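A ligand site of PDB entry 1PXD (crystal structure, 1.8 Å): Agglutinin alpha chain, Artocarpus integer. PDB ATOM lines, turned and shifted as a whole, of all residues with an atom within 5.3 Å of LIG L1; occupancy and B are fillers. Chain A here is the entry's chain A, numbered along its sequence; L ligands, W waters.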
ATOM      1  N   GLY A   1     -27.400 -24.098  25.955  1.00  0.00           N
ATOM      2  CA  GLY A   1     -28.836 -23.871  25.546  1.00  0.00           C
ATOM      3  C   GLY A   1     -29.268 -24.608  24.294  1.00  0.00           C
ATOM      4  O   GLY A   1     -28.470 -25.284  23.650  1.00  0.00           O
ATOM      5  N   LYS A   2     -30.538 -24.477  23.960  1.00  0.00           N
ATOM      6  CA  LYS A   2     -31.085 -25.125  22.772  1.00  0.00           C
ATOM      7  C   LYS A   2     -30.931 -24.159  21.587  1.00  0.00           C
ATOM      8  O   LYS A   2     -31.539 -23.091  21.568  1.00  0.00           O
ATOM      9  CB  LYS A   2     -32.568 -25.466  22.990  1.00  0.00           C
ATOM     10  CG  LYS A   2     -33.174 -26.310  21.907  1.00  0.00           C
ATOM     11  CD  LYS A   2     -34.613 -26.712  22.261  1.00  0.00           C
ATOM     12  CE  LYS A   2     -35.164 -27.704  21.240  1.00  0.00           C
ATOM     13  NZ  LYS A   2     -36.532 -28.154  21.601  1.00  0.00           N
ATOM     14  N   ALA A   3     -30.116 -24.563  20.613  1.00  0.00           N
ATOM     15  CA  ALA A   3     -29.862 -23.759  19.430  1.00  0.00           C
ATOM     16  C   ALA A   3     -31.059 -23.682  18.506  1.00  0.00           C
ATOM     17  O   ALA A   3     -31.854 -24.619  18.414  1.00  0.00           O
ATOM     18  CB  ALA A   3     -28.664 -24.339  18.662  1.00  0.00           C
ATOM     19  N   LYS A  45     -38.630 -20.763  23.131  1.00  0.00           N
ATOM     20  CA  LYS A  45     -38.933 -20.526  24.545  1.00  0.00           C
ATOM     21  C   LYS A  45     -37.899 -20.929  25.582  1.00  0.00           C
ATOM     22  O   LYS A  45     -37.204 -21.937  25.423  1.00  0.00           O
ATOM     23  CB  LYS A  45     -40.255 -21.227  24.884  1.00  0.00           C
ATOM     24  CG  LYS A  45     -41.475 -20.694  24.131  1.00  0.00           C
ATOM     25  CD  LYS A  45     -42.123 -19.528  24.873  1.00  0.00           C
ATOM     26  CE  LYS A  45     -42.730 -19.994  26.191  1.00  0.00           C
ATOM     27  NZ  LYS A  45     -43.262 -18.871  27.026  1.00  0.00           N
ATOM     28  N   SER A  46     -37.831 -20.135  26.648  1.00  0.00           N
ATOM     29  CA  SER A  46     -36.949 -20.409  27.779  1.00  0.00           C
ATOM     30  C   SER A  46     -37.458 -21.641  28.497  1.00  0.00           C
ATOM     31  O   SER A  46     -38.655 -21.962  28.416  1.00  0.00           O
ATOM     32  CB  SER A  46     -36.988 -19.248  28.774  1.00  0.00           C
ATOM     33  OG  SER A  46     -36.428 -19.627  30.024  1.00  0.00           O
ATOM     34  N   PHE A  47     -36.573 -22.335  29.195  1.00  0.00           N
ATOM     35  CA  PHE A  47     -36.957 -23.526  29.945  1.00  0.00           C
ATOM     36  C   PHE A  47     -37.792 -23.128  31.161  1.00  0.00           C
ATOM     37  O   PHE A  47     -38.622 -23.904  31.639  1.00  0.00           O
ATOM     38  CB  PHE A  47     -35.713 -24.317  30.373  1.00  0.00           C
ATOM     39  CG  PHE A  47     -36.011 -25.554  31.170  1.00  0.00           C
ATOM     40  CD1 PHE A  47     -36.051 -25.518  32.558  1.00  0.00           C
ATOM     41  CD2 PHE A  47     -36.284 -26.757  30.529  1.00  0.00           C
ATOM     42  CE1 PHE A  47     -36.358 -26.659  33.297  1.00  0.00           C
ATOM     43  CE2 PHE A  47     -36.596 -27.914  31.263  1.00  0.00           C
ATOM     44  CZ  PHE A  47     -36.630 -27.852  32.643  1.00  0.00           C
ATOM     45  N   VAL A  75     -25.040 -14.057  34.133  1.00  0.00           N
ATOM     46  CA  VAL A  75     -26.212 -14.366  34.931  1.00  0.00           C
ATOM     47  C   VAL A  75     -26.020 -15.803  35.381  1.00  0.00           C
ATOM     48  O   VAL A  75     -25.965 -16.713  34.555  1.00  0.00           O
ATOM     49  CB  VAL A  75     -27.541 -14.252  34.134  1.00  0.00           C
ATOM     50  CG1 VAL A  75     -28.732 -14.671  35.022  1.00  0.00           C
ATOM     51  CG2 VAL A  75     -27.735 -12.818  33.675  1.00  0.00           C
ATOM     52  N   SER A  76     -25.881 -15.985  36.694  1.00  0.00           N
ATOM     53  CA  SER A  76     -25.676 -17.310  37.280  1.00  0.00           C
ATOM     54  C   SER A  76     -24.513 -18.097  36.688  1.00  0.00           C
ATOM     55  O   SER A  76     -24.641 -19.297  36.429  1.00  0.00           O
ATOM     56  CB  SER A  76     -26.955 -18.139  37.176  1.00  0.00           C
ATOM     57  OG  SER A  76     -28.023 -17.528  37.882  1.00  0.00           O
ATOM     58  N   TYR A  78     -23.105 -17.903  33.634  1.00  0.00           N
ATOM     59  CA  TYR A  78     -22.989 -17.933  32.172  1.00  0.00           C
ATOM     60  C   TYR A  78     -23.265 -16.595  31.493  1.00  0.00           C
ATOM     61  O   TYR A  78     -24.009 -15.766  32.015  1.00  0.00           O
ATOM     62  CB  TYR A  78     -23.913 -19.009  31.596  1.00  0.00           C
ATOM     63  CG  TYR A  78     -23.543 -20.416  32.006  1.00  0.00           C
ATOM     64  CD1 TYR A  78     -24.199 -21.048  33.053  1.00  0.00           C
ATOM     65  CD2 TYR A  78     -22.510 -21.091  31.359  1.00  0.00           C
ATOM     66  CE1 TYR A  78     -23.833 -22.338  33.451  1.00  0.00           C
ATOM     67  CE2 TYR A  78     -22.134 -22.363  31.749  1.00  0.00           C
ATOM     68  CZ  TYR A  78     -22.795 -22.986  32.795  1.00  0.00           C
ATOM     69  OH  TYR A  78     -22.406 -24.248  33.200  1.00  0.00           O
ATOM     70  N   ILE A 120     -31.183 -20.661  23.262  1.00  0.00           N
ATOM     71  CA  ILE A 120     -31.856 -20.282  24.508  1.00  0.00           C
ATOM     72  C   ILE A 120     -31.881 -21.471  25.462  1.00  0.00           C
ATOM     73  O   ILE A 120     -32.293 -22.566  25.068  1.00  0.00           O
ATOM     74  CB  ILE A 120     -33.321 -19.834  24.267  1.00  0.00           C
ATOM     75  CG1 ILE A 120     -33.354 -18.561  23.420  1.00  0.00           C
ATOM     76  CG2 ILE A 120     -34.018 -19.592  25.612  1.00  0.00           C
ATOM     77  CD1 ILE A 120     -34.756 -18.129  23.008  1.00  0.00           C
ATOM     78  N   GLY A 121     -31.412 -21.235  26.691  1.00  0.00           N
ATOM     79  CA  GLY A 121     -31.405 -22.258  27.727  1.00  0.00           C
ATOM     80  C   GLY A 121     -32.446 -21.751  28.703  1.00  0.00           C
ATOM     81  O   GLY A 121     -33.640 -22.022  28.522  1.00  0.00           O
ATOM     82  N   TYR A 122     -32.018 -21.024  29.724  1.00  0.00           N
ATOM     83  CA  TYR A 122     -32.955 -20.418  30.646  1.00  0.00           C
ATOM     84  C   TYR A 122     -33.179 -19.035  30.038  1.00  0.00           C
ATOM     85  O   TYR A 122     -34.275 -18.467  30.111  1.00  0.00           O
ATOM     86  CB  TYR A 122     -32.343 -20.256  32.046  1.00  0.00           C
ATOM     87  CG  TYR A 122     -32.624 -21.386  33.011  1.00  0.00           C
ATOM     88  CD1 TYR A 122     -32.813 -22.702  32.554  1.00  0.00           C
ATOM     89  CD2 TYR A 122     -32.647 -21.158  34.393  1.00  0.00           C
ATOM     90  CE1 TYR A 122     -33.027 -23.759  33.460  1.00  0.00           C
ATOM     91  CE2 TYR A 122     -32.852 -22.207  35.305  1.00  0.00           C
ATOM     92  CZ  TYR A 122     -33.035 -23.497  34.839  1.00  0.00           C
ATOM     93  OH  TYR A 122     -33.207 -24.526  35.737  1.00  0.00           O
ATOM     94  N   TRP A 123     -32.119 -18.513  29.408  1.00  0.00           N
ATOM     95  CA  TRP A 123     -32.156 -17.200  28.786  1.00  0.00           C
ATOM     96  C   TRP A 123     -31.517 -17.256  27.400  1.00  0.00           C
ATOM     97  O   TRP A 123     -30.922 -18.267  26.998  1.00  0.00           O
ATOM     98  CB  TRP A 123     -31.385 -16.190  29.643  1.00  0.00           C
ATOM     99  CG  TRP A 123     -31.868 -16.122  31.063  1.00  0.00           C
ATOM    100  CD1 TRP A 123     -33.007 -15.507  31.518  1.00  0.00           C
ATOM    101  CD2 TRP A 123     -31.274 -16.762  32.189  1.00  0.00           C
ATOM    102  NE1 TRP A 123     -33.157 -15.746  32.863  1.00  0.00           N
ATOM    103  CE2 TRP A 123     -32.102 -16.505  33.305  1.00  0.00           C
ATOM    104  CE3 TRP A 123     -30.110 -17.529  32.372  1.00  0.00           C
ATOM    105  CZ2 TRP A 123     -31.821 -16.984  34.576  1.00  0.00           C
ATOM    106  CZ3 TRP A 123     -29.821 -18.004  33.639  1.00  0.00           C
ATOM    107  CH2 TRP A 123     -30.672 -17.731  34.724  1.00  0.00           C
HETATM  108  C1  LIG L   1     -30.875 -24.898  30.481  1.00  0.00           C
HETATM  109  C2  LIG L   1     -31.670 -25.503  29.597  1.00  0.00           C
HETATM  110  C3  LIG L   1     -30.857 -26.025  28.562  1.00  0.00           C
HETATM  111  N1  LIG L   1     -29.534 -25.725  28.854  1.00  0.00           N
HETATM  112  C4  LIG L   1     -29.532 -25.010  30.033  1.00  0.00           C
HETATM  113  C5  LIG L   1     -31.286 -26.733  27.418  1.00  0.00           C
HETATM  114  C6  LIG L   1     -30.462 -27.283  26.399  1.00  0.00           C
HETATM  115  C7  LIG L   1     -30.895 -27.996  25.236  1.00  0.00           C
HETATM  116  C8  LIG L   1     -29.815 -28.369  24.522  1.00  0.00           C
HETATM  117  C9  LIG L   1     -28.640 -27.901  25.185  1.00  0.00           C
HETATM  118  N2  LIG L   1     -29.054 -27.225  26.357  1.00  0.00           N
HETATM  119  C10 LIG L   1     -27.280 -28.073  24.750  1.00  0.00           C
HETATM  120  C11 LIG L   1     -26.123 -27.556  25.414  1.00  0.00           C
HETATM  121  C12 LIG L   1     -24.759 -27.698  25.002  1.00  0.00           C
HETATM  122  C13 LIG L   1     -23.965 -27.034  25.880  1.00  0.00           C
HETATM  123  C14 LIG L   1     -24.805 -26.463  26.864  1.00  0.00           C
HETATM  124  N3  LIG L   1     -26.124 -26.809  26.574  1.00  0.00           N
HETATM  125  C15 LIG L   1     -24.387 -25.672  27.954  1.00  0.00           C
HETATM  126  C16 LIG L   1     -25.240 -25.122  28.937  1.00  0.00           C
HETATM  127  C17 LIG L   1     -24.839 -24.318  30.038  1.00  0.00           C
HETATM  128  C18 LIG L   1     -25.900 -24.018  30.748  1.00  0.00           C
HETATM  129  C19 LIG L   1     -27.047 -24.593  30.142  1.00  0.00           C
HETATM  130  N4  LIG L   1     -26.629 -25.275  29.002  1.00  0.00           N
HETATM  131  C20 LIG L   1     -28.397 -24.480  30.634  1.00  0.00           C
HETATM  132  C21 LIG L   1     -20.154 -24.610  28.152  1.00  0.00           C
HETATM  133  C22 LIG L   1     -21.018 -23.915  27.267  1.00  0.00           C
HETATM  134  C23 LIG L   1     -22.363 -24.269  27.231  1.00  0.00           C
HETATM  135  C24 LIG L   1     -22.872 -25.359  28.100  1.00  0.00           C
HETATM  136  C25 LIG L   1     -21.984 -26.050  28.989  1.00  0.00           C
HETATM  137  C26 LIG L   1     -20.621 -25.673  29.013  1.00  0.00           C
HETATM  138  C27 LIG L   1     -27.126 -30.292  23.333  1.00  0.00           C
HETATM  139  C28 LIG L   1     -26.855 -30.915  22.105  1.00  0.00           C
HETATM  140  C29 LIG L   1     -26.456 -30.127  20.977  1.00  0.00           C
HETATM  141  C30 LIG L   1     -26.330 -28.711  21.045  1.00  0.00           C
HETATM  142  C31 LIG L   1     -26.600 -28.067  22.245  1.00  0.00           C
HETATM  143  C32 LIG L   1     -27.012 -28.856  23.430  1.00  0.00           C
HETATM  144  C33 LIG L   1     -28.689 -22.422  34.461  1.00  0.00           C
HETATM  145  C34 LIG L   1     -29.025 -21.663  33.293  1.00  0.00           C
HETATM  146  C35 LIG L   1     -28.962 -22.287  32.017  1.00  0.00           C
HETATM  147  C36 LIG L   1     -28.553 -23.693  31.958  1.00  0.00           C
HETATM  148  C37 LIG L   1     -28.236 -24.421  33.186  1.00  0.00           C
HETATM  149  C38 LIG L   1     -28.308 -23.788  34.397  1.00  0.00           C
HETATM  150  C39 LIG L   1     -33.444 -28.215  27.500  1.00  0.00           C
HETATM  151  C40 LIG L   1     -32.815 -26.927  27.240  1.00  0.00           C
HETATM  152  C41 LIG L   1     -33.604 -25.786  26.773  1.00  0.00           C
HETATM  153  C42 LIG L   1     -34.997 -25.950  26.576  1.00  0.00           C
HETATM  154  C43 LIG L   1     -35.586 -27.214  26.819  1.00  0.00           C
HETATM  155  C44 LIG L   1     -34.831 -28.342  27.280  1.00  0.00           C
HETATM  156  S1  LIG L   1     -18.486 -24.161  28.179  1.00  0.00           S
HETATM  157  O1  LIG L   1     -17.879 -24.674  29.371  1.00  0.00           O
HETATM  158  O2  LIG L   1     -18.469 -22.754  28.180  1.00  0.00           O
HETATM  159  O3  LIG L   1     -17.836 -24.715  26.915  1.00  0.00           O
HETATM  160  S2  LIG L   1     -26.108 -30.941  19.475  1.00  0.00           S
HETATM  161  O4  LIG L   1     -25.719 -30.001  18.455  1.00  0.00           O
HETATM  162  O5  LIG L   1     -27.304 -31.655  19.082  1.00  0.00           O
HETATM  163  O6  LIG L   1     -24.948 -31.902  19.780  1.00  0.00           O
HETATM  164  S3  LIG L   1     -28.736 -21.663  36.035  1.00  0.00           S
HETATM  165  O7  LIG L   1     -28.380 -22.600  37.048  1.00  0.00           O
HETATM  166  O8  LIG L   1     -30.063 -21.187  36.223  1.00  0.00           O
HETATM  167  O9  LIG L   1     -27.734 -20.518  36.006  1.00  0.00           O
HETATM  168  S4  LIG L   1     -37.293 -27.417  26.559  1.00  0.00           S
HETATM  169  O10 LIG L   1     -37.699 -28.540  27.295  1.00  0.00           O
HETATM  170  O11 LIG L   1     -37.524 -27.624  25.167  1.00  0.00           O
HETATM  171  O12 LIG L   1     -37.966 -26.165  27.068  1.00  0.00           O
HETATM  172  C1  LG2 L   2     -27.936 -29.676  30.283  1.00  0.00           C
HETATM  173  C2  LG2 L   2     -28.765 -30.298  29.444  1.00  0.00           C
HETATM  174  C3  LG2 L   2     -28.019 -30.946  28.452  1.00  0.00           C
HETATM  175  N1  LG2 L   2     -26.662 -30.653  28.695  1.00  0.00           N
HETATM  176  C4  LG2 L   2     -26.605 -29.879  29.854  1.00  0.00           C
HETATM  177  C5  LG2 L   2     -28.524 -31.753  27.397  1.00  0.00           C
HETATM  178  C6  LG2 L   2     -27.737 -32.421  26.412  1.00  0.00           C
HETATM  179  C7  LG2 L   2     -28.231 -33.266  25.387  1.00  0.00           C
HETATM  180  C8  LG2 L   2     -27.210 -33.727  24.670  1.00  0.00           C
HETATM  181  C9  LG2 L   2     -25.994 -33.189  25.206  1.00  0.00           C
HETATM  182  N2  LG2 L   2     -26.337 -32.377  26.300  1.00  0.00           N
HETATM  183  C10 LG2 L   2     -24.659 -33.446  24.707  1.00  0.00           C
HETATM  184  C11 LG2 L   2     -23.455 -32.901  25.254  1.00  0.00           C
HETATM  185  C12 LG2 L   2     -22.127 -33.112  24.775  1.00  0.00           C
HETATM  186  C13 LG2 L   2     -21.264 -32.422  25.586  1.00  0.00           C
HETATM  187  C14 LG2 L   2     -22.029 -31.763  26.580  1.00  0.00           C
HETATM  188  N3  LG2 L   2     -23.379 -32.072  26.361  1.00  0.00           N
HETATM  189  C15 LG2 L   2     -21.539 -30.963  27.650  1.00  0.00           C
HETATM  190  C16 LG2 L   2     -22.344 -30.339  28.675  1.00  0.00           C
HETATM  191  C17 LG2 L   2     -21.851 -29.571  29.765  1.00  0.00           C
HETATM  192  C18 LG2 L   2     -22.866 -29.173  30.521  1.00  0.00           C
HETATM  193  C19 LG2 L   2     -24.077 -29.640  29.952  1.00  0.00           C
HETATM  194  N4  LG2 L   2     -23.739 -30.367  28.791  1.00  0.00           N
HETATM  195  C20 LG2 L   2     -25.415 -29.407  30.469  1.00  0.00           C
HETATM  196  C21 LG2 L   2     -17.164 -30.403  27.919  1.00  0.00           C
HETATM  197  C22 LG2 L   2     -17.757 -31.501  28.607  1.00  0.00           C
HETATM  198  C23 LG2 L   2     -19.164 -31.684  28.525  1.00  0.00           C
HETATM  199  C24 LG2 L   2     -19.981 -30.738  27.737  1.00  0.00           C
HETATM  200  C25 LG2 L   2     -19.351 -29.639  27.051  1.00  0.00           C
HETATM  201  C26 LG2 L   2     -17.944 -29.466  27.146  1.00  0.00           C
HETATM  202  C27 LG2 L   2     -24.445 -33.962  22.103  1.00  0.00           C
HETATM  203  C28 LG2 L   2     -24.331 -34.952  21.094  1.00  0.00           C
HETATM  204  C29 LG2 L   2     -24.323 -36.357  21.450  1.00  0.00           C
HETATM  205  C30 LG2 L   2     -24.416 -36.787  22.795  1.00  0.00           C
HETATM  206  C31 LG2 L   2     -24.527 -35.842  23.806  1.00  0.00           C
HETATM  207  C32 LG2 L   2     -24.542 -34.402  23.484  1.00  0.00           C
HETATM  208  C33 LG2 L   2     -25.751 -27.375  34.422  1.00  0.00           C
HETATM  209  C34 LG2 L   2     -26.094 -28.754  34.277  1.00  0.00           C
HETATM  210  C35 LG2 L   2     -25.995 -29.363  33.021  1.00  0.00           C
HETATM  211  C36 LG2 L   2     -25.541 -28.594  31.843  1.00  0.00           C
HETATM  212  C37 LG2 L   2     -25.195 -27.185  32.011  1.00  0.00           C
HETATM  213  C38 LG2 L   2     -25.295 -26.597  33.294  1.00  0.00           C
HETATM  214  C39 LG2 L   2     -30.689 -32.919  28.255  1.00  0.00           C
HETATM  215  C40 LG2 L   2     -30.085 -31.967  27.319  1.00  0.00           C
HETATM  216  C41 LG2 L   2     -30.916 -31.286  26.344  1.00  0.00           C
HETATM  217  C42 LG2 L   2     -32.325 -31.548  26.319  1.00  0.00           C
HETATM  218  C43 LG2 L   2     -32.884 -32.483  27.239  1.00  0.00           C
HETATM  219  C44 LG2 L   2     -32.082 -33.161  28.209  1.00  0.00           C
HETATM  220  S1  LG2 L   2     -15.436 -30.182  28.020  1.00  0.00           S
HETATM  221  O1  LG2 L   2     -15.047 -29.111  27.164  1.00  0.00           O
HETATM  222  O2  LG2 L   2     -14.874 -31.401  27.591  1.00  0.00           O
HETATM  223  O3  LG2 L   2     -15.049 -29.898  29.480  1.00  0.00           O
HETATM  224  S2  LG2 L   2     -24.194 -37.577  20.195  1.00  0.00           S
HETATM  225  O4  LG2 L   2     -24.204 -38.901  20.778  1.00  0.00           O
HETATM  226  O5  LG2 L   2     -22.964 -37.362  19.486  1.00  0.00           O
HETATM  227  O6  LG2 L   2     -25.406 -37.386  19.284  1.00  0.00           O
HETATM  228  S3  LG2 L   2     -25.870 -26.671  36.040  1.00  0.00           S
HETATM  229  O7  LG2 L   2     -25.474 -25.285  36.053  1.00  0.00           O
HETATM  230  O8  LG2 L   2     -24.987 -27.448  36.849  1.00  0.00           O
HETATM  231  O9  LG2 L   2     -27.309 -26.821  36.555  1.00  0.00           O
HETATM  232  S4  LG2 L   2     -34.585 -32.822  27.209  1.00  0.00           S
HETATM  233  O10 LG2 L   2     -34.905 -33.540  28.362  1.00  0.00           O
HETATM  234  O11 LG2 L   2     -34.888 -33.605  26.046  1.00  0.00           O
HETATM  235  O12 LG2 L   2     -35.307 -31.502  27.197  1.00  0.00           O
HETATM  236  O   HOH W   1     -23.691 -21.046  27.544  1.00  0.00           O
HETATM  237  O   HOH W   2     -30.917 -18.911  37.875  1.00  0.00           O
HETATM  238  O   HOH W   3     -26.990 -20.014  30.518  1.00  0.00           O
HETATM  239  O   HOH W   4     -27.243 -22.156  27.914  1.00  0.00           O
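The backbone NH (N) of Gly 1 lies within hydrogen-bond range of a nitrogen (N4) of LIG L1 (3.4 Å).
O of Ser 76 lies close to O9 of LIG L1 (3.4 Å).
Merely in contact with LIG L1: Tyr 122, Tyr 78, Lys 2, Gly 121, Trp 123, Phe 47 and Ile 120.
Hydrophobic or aromatic side chains within 4 Å of LIG L1: Phe 47, Tyr 78, Tyr 122 and Trp 123.
Water W2 bridges O8 of LIG L1 and OG of Ser 76.
Water W4 bridges the backbone NH of Gly 1 (2.8 Å) and a nitrogen (N4) of LIG L1 (3.4 Å).
The backbone carbonyl oxygen (O) of Ile 120 is in hydrogen-bond range of the backbone NH (N) of Lys 2 (2.8 Å).
O of Gly 121 lies within hydrogen-bond range of N of Phe 47 (3.0 Å).
OG of Ser 46 sits at hydrogen-bond distance from O of Tyr 122, at 2.4 Å.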
